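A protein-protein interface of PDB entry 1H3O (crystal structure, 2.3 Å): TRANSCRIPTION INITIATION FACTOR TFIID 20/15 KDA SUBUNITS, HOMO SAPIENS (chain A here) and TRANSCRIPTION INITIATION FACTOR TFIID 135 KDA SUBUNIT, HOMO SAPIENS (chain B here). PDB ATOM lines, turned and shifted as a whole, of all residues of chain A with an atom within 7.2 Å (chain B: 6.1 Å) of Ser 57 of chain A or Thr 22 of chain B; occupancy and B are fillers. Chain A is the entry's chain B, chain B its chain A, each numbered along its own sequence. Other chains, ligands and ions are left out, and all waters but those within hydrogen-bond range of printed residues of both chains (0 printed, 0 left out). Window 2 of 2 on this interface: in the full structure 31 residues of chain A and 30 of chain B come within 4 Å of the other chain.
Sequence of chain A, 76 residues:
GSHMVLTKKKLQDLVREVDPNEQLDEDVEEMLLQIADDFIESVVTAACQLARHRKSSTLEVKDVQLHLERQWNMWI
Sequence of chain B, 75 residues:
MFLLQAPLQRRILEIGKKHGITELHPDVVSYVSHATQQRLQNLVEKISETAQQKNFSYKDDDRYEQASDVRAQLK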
ATOM      1  N   CYS A  48     -18.392  31.436  -2.431  1.00  0.00           N
ATOM      2  CA  CYS A  48     -17.173  30.926  -1.817  1.00  0.00           C
ATOM      3  C   CYS A  48     -17.150  31.257  -0.334  1.00  0.00           C
ATOM      4  O   CYS A  48     -16.621  30.494   0.474  1.00  0.00           O
ATOM      5  CB  CYS A  48     -15.943  31.517  -2.502  1.00  0.00           C
ATOM      6  SG  CYS A  48     -15.670  30.819  -4.134  1.00  0.00           S
ATOM      7  N   ALA A  51     -19.467  28.811   1.386  1.00  0.00           N
ATOM      8  CA  ALA A  51     -18.772  27.532   1.427  1.00  0.00           C
ATOM      9  C   ALA A  51     -17.728  27.538   2.530  1.00  0.00           C
ATOM     10  O   ALA A  51     -17.737  26.682   3.414  1.00  0.00           O
ATOM     11  CB  ALA A  51     -18.107  27.254   0.092  1.00  0.00           C
ATOM     12  N   ARG A  52     -16.827  28.511   2.474  1.00  0.00           N
ATOM     13  CA  ARG A  52     -15.780  28.622   3.474  1.00  0.00           C
ATOM     14  C   ARG A  52     -16.416  28.577   4.861  1.00  0.00           C
ATOM     15  O   ARG A  52     -15.839  28.024   5.794  1.00  0.00           O
ATOM     16  CB  ARG A  52     -15.011  29.934   3.294  1.00  0.00           C
ATOM     17  CG  ARG A  52     -13.531  29.835   3.636  1.00  0.00           C
ATOM     18  CD  ARG A  52     -12.887  31.208   3.790  1.00  0.00           C
ATOM     19  NE  ARG A  52     -13.447  31.940   4.925  1.00  0.00           N
ATOM     20  CZ  ARG A  52     -12.938  33.065   5.423  1.00  0.00           C
ATOM     21  NH1 ARG A  52     -11.847  33.601   4.889  1.00  0.00           N
ATOM     22  NH2 ARG A  52     -13.519  33.652   6.462  1.00  0.00           N
ATOM     23  N   ARG A  54     -19.124  26.937   5.728  1.00  0.00           N
ATOM     24  CA  ARG A  54     -19.485  25.551   6.017  1.00  0.00           C
ATOM     25  C   ARG A  54     -18.230  24.840   6.504  1.00  0.00           C
ATOM     26  O   ARG A  54     -18.244  23.626   6.718  1.00  0.00           O
ATOM     27  CB  ARG A  54     -19.953  24.818   4.756  1.00  0.00           C
ATOM     28  CG  ARG A  54     -21.238  25.293   4.113  1.00  0.00           C
ATOM     29  CD  ARG A  54     -21.592  24.335   2.982  1.00  0.00           C
ATOM     30  NE  ARG A  54     -20.521  24.248   1.990  1.00  0.00           N
ATOM     31  CZ  ARG A  54     -20.367  23.245   1.127  1.00  0.00           C
ATOM     32  NH1 ARG A  54     -21.206  22.217   1.128  1.00  0.00           N
ATOM     33  NH2 ARG A  54     -19.383  23.276   0.242  1.00  0.00           N
ATOM     34  N   LYS A  55     -17.145  25.597   6.657  1.00  0.00           N
ATOM     35  CA  LYS A  55     -15.870  25.034   7.078  1.00  0.00           C
ATOM     36  C   LYS A  55     -15.426  24.111   5.947  1.00  0.00           C
ATOM     37  O   LYS A  55     -14.769  23.096   6.174  1.00  0.00           O
ATOM     38  CB  LYS A  55     -16.038  24.232   8.372  1.00  0.00           C
ATOM     39  CG  LYS A  55     -16.612  25.028   9.533  1.00  0.00           C
ATOM     40  CD  LYS A  55     -15.683  26.163   9.937  1.00  0.00           C
ATOM     41  CE  LYS A  55     -16.182  26.873  11.190  1.00  0.00           C
ATOM     42  NZ  LYS A  55     -17.543  27.462  11.010  1.00  0.00           N
ATOM     43  N   SER A  56     -15.808  24.478   4.726  1.00  0.00           N
ATOM     44  CA  SER A  56     -15.477  23.697   3.538  1.00  0.00           C
ATOM     45  C   SER A  56     -14.437  24.384   2.656  1.00  0.00           C
ATOM     46  O   SER A  56     -13.948  25.472   2.972  1.00  0.00           O
ATOM     47  CB  SER A  56     -16.742  23.444   2.721  1.00  0.00           C
ATOM     48  OG  SER A  56     -16.456  22.679   1.565  1.00  0.00           O
ATOM     49  N   SER A  57     -14.111  23.742   1.541  1.00  0.00           N
ATOM     50  CA  SER A  57     -13.130  24.278   0.610  1.00  0.00           C
ATOM     51  C   SER A  57     -13.505  23.939  -0.821  1.00  0.00           C
ATOM     52  O   SER A  57     -12.787  24.292  -1.758  1.00  0.00           O
ATOM     53  CB  SER A  57     -11.743  23.710   0.916  1.00  0.00           C
ATOM     54  OG  SER A  57     -11.717  22.301   0.749  1.00  0.00           O
ATOM     55  N   THR A  58     -14.615  23.225  -0.983  1.00  0.00           N
ATOM     56  CA  THR A  58     -15.109  22.857  -2.306  1.00  0.00           C
ATOM     57  C   THR A  58     -16.371  23.659  -2.604  1.00  0.00           C
ATOM     58  O   THR A  58     -17.331  23.631  -1.827  1.00  0.00           O
ATOM     59  CB  THR A  58     -15.462  21.364  -2.398  1.00  0.00           C
ATOM     60  OG1 THR A  58     -14.282  20.575  -2.206  1.00  0.00           O
ATOM     61  CG2 THR A  58     -16.051  21.050  -3.768  1.00  0.00           C
ATOM     62  N   LEU A  59     -16.365  24.380  -3.722  1.00  0.00           N
ATOM     63  CA  LEU A  59     -17.516  25.184  -4.106  1.00  0.00           C
ATOM     64  C   LEU A  59     -18.613  24.257  -4.596  1.00  0.00           C
ATOM     65  O   LEU A  59     -18.378  23.406  -5.460  1.00  0.00           O
ATOM     66  CB  LEU A  59     -17.154  26.164  -5.224  1.00  0.00           C
ATOM     67  CG  LEU A  59     -17.659  27.613  -5.106  1.00  0.00           C
ATOM     68  CD1 LEU A  59     -17.678  28.238  -6.501  1.00  0.00           C
ATOM     69  CD2 LEU A  59     -19.047  27.669  -4.491  1.00  0.00           C
ATOM     70  N   GLU A  60     -19.811  24.421  -4.042  1.00  0.00           N
ATOM     71  CA  GLU A  60     -20.941  23.596  -4.441  1.00  0.00           C
ATOM     72  C   GLU A  60     -22.198  24.412  -4.730  1.00  0.00           C
ATOM     73  O   GLU A  60     -22.403  25.479  -4.149  1.00  0.00           O
ATOM     74  CB  GLU A  60     -21.237  22.576  -3.354  1.00  0.00           C
ATOM     75  CG  GLU A  60     -20.020  21.810  -2.900  1.00  0.00           C
ATOM     76  CD  GLU A  60     -20.390  20.590  -2.106  1.00  0.00           C
ATOM     77  OE1 GLU A  60     -20.976  19.663  -2.708  1.00  0.00           O
ATOM     78  OE2 GLU A  60     -20.102  20.562  -0.889  1.00  0.00           O
ATOM     79  N   LEU B  13     -12.880  28.874 -10.933  1.00  0.00           N
ATOM     80  CA  LEU B  13     -11.768  28.301 -10.192  1.00  0.00           C
ATOM     81  C   LEU B  13     -10.836  29.424  -9.755  1.00  0.00           C
ATOM     82  O   LEU B  13     -10.322  29.420  -8.633  1.00  0.00           O
ATOM     83  CB  LEU B  13     -11.006  27.304 -11.076  1.00  0.00           C
ATOM     84  CG  LEU B  13     -11.650  25.929 -11.289  1.00  0.00           C
ATOM     85  CD1 LEU B  13     -11.214  25.330 -12.628  1.00  0.00           C
ATOM     86  CD2 LEU B  13     -11.271  25.023 -10.134  1.00  0.00           C
ATOM     87  N   GLY B  16     -12.205  31.548  -6.879  1.00  0.00           N
ATOM     88  CA  GLY B  16     -12.159  30.765  -5.656  1.00  0.00           C
ATOM     89  C   GLY B  16     -10.824  30.839  -4.934  1.00  0.00           C
ATOM     90  O   GLY B  16     -10.787  30.972  -3.710  1.00  0.00           O
ATOM     91  N   LYS B  17      -9.726  30.756  -5.684  1.00  0.00           N
ATOM     92  CA  LYS B  17      -8.395  30.820  -5.087  1.00  0.00           C
ATOM     93  C   LYS B  17      -8.258  32.013  -4.166  1.00  0.00           C
ATOM     94  O   LYS B  17      -7.653  31.914  -3.104  1.00  0.00           O
ATOM     95  CB  LYS B  17      -7.317  30.900  -6.159  1.00  0.00           C
ATOM     96  CG  LYS B  17      -6.955  29.571  -6.760  1.00  0.00           C
ATOM     97  CD  LYS B  17      -5.865  29.745  -7.803  1.00  0.00           C
ATOM     98  CE  LYS B  17      -5.426  28.405  -8.371  1.00  0.00           C
ATOM     99  NZ  LYS B  17      -4.749  27.578  -7.337  1.00  0.00           N
ATOM    100  N   GLY B  20     -10.440  31.319  -0.246  1.00  0.00           N
ATOM    101  CA  GLY B  20     -10.366  30.059   0.467  1.00  0.00           C
ATOM    102  C   GLY B  20     -10.929  28.824  -0.198  1.00  0.00           C
ATOM    103  O   GLY B  20     -11.135  27.815   0.471  1.00  0.00           O
ATOM    104  N   ILE B  21     -11.173  28.877  -1.498  1.00  0.00           N
ATOM    105  CA  ILE B  21     -11.712  27.710  -2.170  1.00  0.00           C
ATOM    106  C   ILE B  21     -10.673  27.029  -3.019  1.00  0.00           C
ATOM    107  O   ILE B  21     -10.011  27.659  -3.838  1.00  0.00           O
ATOM    108  CB  ILE B  21     -12.932  28.064  -3.033  1.00  0.00           C
ATOM    109  CG1 ILE B  21     -14.108  28.398  -2.116  1.00  0.00           C
ATOM    110  CG2 ILE B  21     -13.268  26.910  -3.974  1.00  0.00           C
ATOM    111  CD1 ILE B  21     -14.387  27.337  -1.059  1.00  0.00           C
ATOM    112  N   THR B  22     -10.562  25.722  -2.821  1.00  0.00           N
ATOM    113  CA  THR B  22      -9.584  24.912  -3.519  1.00  0.00           C
ATOM    114  C   THR B  22     -10.202  24.113  -4.649  1.00  0.00           C
ATOM    115  O   THR B  22      -9.578  23.916  -5.689  1.00  0.00           O
ATOM    116  CB  THR B  22      -8.915  23.939  -2.542  1.00  0.00           C
ATOM    117  OG1 THR B  22      -8.804  24.559  -1.253  1.00  0.00           O
ATOM    118  CG2 THR B  22      -7.529  23.578  -3.040  1.00  0.00           C
ATOM    119  N   GLU B  23     -11.424  23.637  -4.435  1.00  0.00           N
ATOM    120  CA  GLU B  23     -12.120  22.857  -5.452  1.00  0.00           C
ATOM    121  C   GLU B  23     -13.558  23.326  -5.643  1.00  0.00           C
ATOM    122  O   GLU B  23     -14.066  24.139  -4.875  1.00  0.00           O
ATOM    123  CB  GLU B  23     -12.110  21.369  -5.081  1.00  0.00           C
ATOM    124  CG  GLU B  23     -10.878  20.612  -5.568  1.00  0.00           C
ATOM    125  CD  GLU B  23     -10.872  19.142  -5.159  1.00  0.00           C
ATOM    126  OE1 GLU B  23     -11.892  18.449  -5.379  1.00  0.00           O
ATOM    127  OE2 GLU B  23      -9.839  18.678  -4.627  1.00  0.00           O
ATOM    128  N   LEU B  24     -14.204  22.812  -6.680  1.00  0.00           N
ATOM    129  CA  LEU B  24     -15.586  23.161  -6.959  1.00  0.00           C
ATOM    130  C   LEU B  24     -16.288  21.965  -7.590  1.00  0.00           C
ATOM    131  O   LEU B  24     -15.752  21.320  -8.494  1.00  0.00           O
ATOM    132  CB  LEU B  24     -15.655  24.382  -7.889  1.00  0.00           C
ATOM    133  CG  LEU B  24     -15.068  24.305  -9.302  1.00  0.00           C
ATOM    134  CD1 LEU B  24     -16.056  23.647 -10.253  1.00  0.00           C
ATOM    135  CD2 LEU B  24     -14.761  25.710  -9.784  1.00  0.00           C
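N of Leu 59 of chain A sits at hydrogen-bond distance from O of Glu 23 of chain B, 2.6 Å away.
The backbone NH of Thr 22 of chain B is in hydrogen-bond range of the backbone carbonyl oxygen of Ser 57 of chain A.
N of Glu 23 of chain B is in hydrogen-bond range of O of Ser 57 of chain A (3.1 Å).
The backbone carbonyl oxygen (O) of Gly 16 of chain B is in hydrogen-bond range of the backbone NH (N) of Ile 21 of chain B, 3.1 Å away.
The side-chain hydroxyl of Ser 56 of chain A is in hydrogen-bond range of the backbone NH of Thr 58 of chain A, at 3.2 Å.
The guanidinium group of Arg 54 of chain A lies within hydrogen-bond range of the backbone carbonyl oxygen of Thr 58 of chain A, 2.9 Å away.
The backbone carbonyl oxygen (O) of Ala 51 of chain A sits at hydrogen-bond distance from the backbone NH (N) of Ser 56 of chain A (3.2 Å).
Cys 48 of chain A touches Gly 16 of chain B (SG to CA, 3.8 Å).
CG1 of Ile 21 of chain B touches SG of Cys 48 of chain A (3.5 Å).
Ala 51 of chain A touches Ile 21 of chain B.
Ser 57 of chain A touches Ile 21 of chain B (O to CG2, 3.5 Å).
Thr 58 of chain A touches Glu 23 of chain B.
CG2 of Thr 58 of chain A touches CA of Leu 24 of chain B, 3.9 Å away.
Leu 24 of chain B touches Leu 59 of chain A (CA to O, 3.2 Å).
Of the printed residues of chain B, Cys 48 of chain A touches Gly 16 and Ile 21.
Ser 56 of chain A touches none of the printed residues of chain B.
Ser 57 of chain A touches just these residues of chain B: Ile 21, Thr 22 and Glu 23.
Of the printed residues of chain B, Thr 58 of chain A touches Glu 23 and Leu 24.
Printed residues of chain A within 4 Å of Gly 16 of chain B: Cys 48.
Lys 17 of chain B touches none of the printed residues of chain A.
Printed residues of chain A within 4 Å of Ile 21 of chain B: Cys 48, Ala 51 and Ser 57.
Of the printed residues of chain A, Thr 22 of chain B touches Ser 57 (2.9 Å).
Of the printed residues of chain A, Glu 23 of chain B touches Ser 57, Thr 58 and Leu 59.
The nearest residue of chain B that does not touch Ser 57 of chain A is Gly 20 of chain B (4.1 Å).
The nearest residue of chain A that does not touch Thr 22 of chain B is Thr 58 of chain A (5.1 Å).
Of the 10 printed residues of chain A, 5 touch a printed residue of chain B.
Printed residues of chain A that touch a printed residue of chain B: Cys 48, Ala 51, Ser 57, Thr 58 and Leu 59.
Hydrophobic or aromatic side chains of chain A that line the printed part of chain B: Ala 51 and Leu 59.
Hydrophobic or aromatic side chains of chain B that line the printed part of chain A: Ile 21 and Leu 24.
Among the printed residues, no Asp or Glu carboxylate lies within 4 Å of a Lys or Arg side-chain nitrogen of the other chain.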
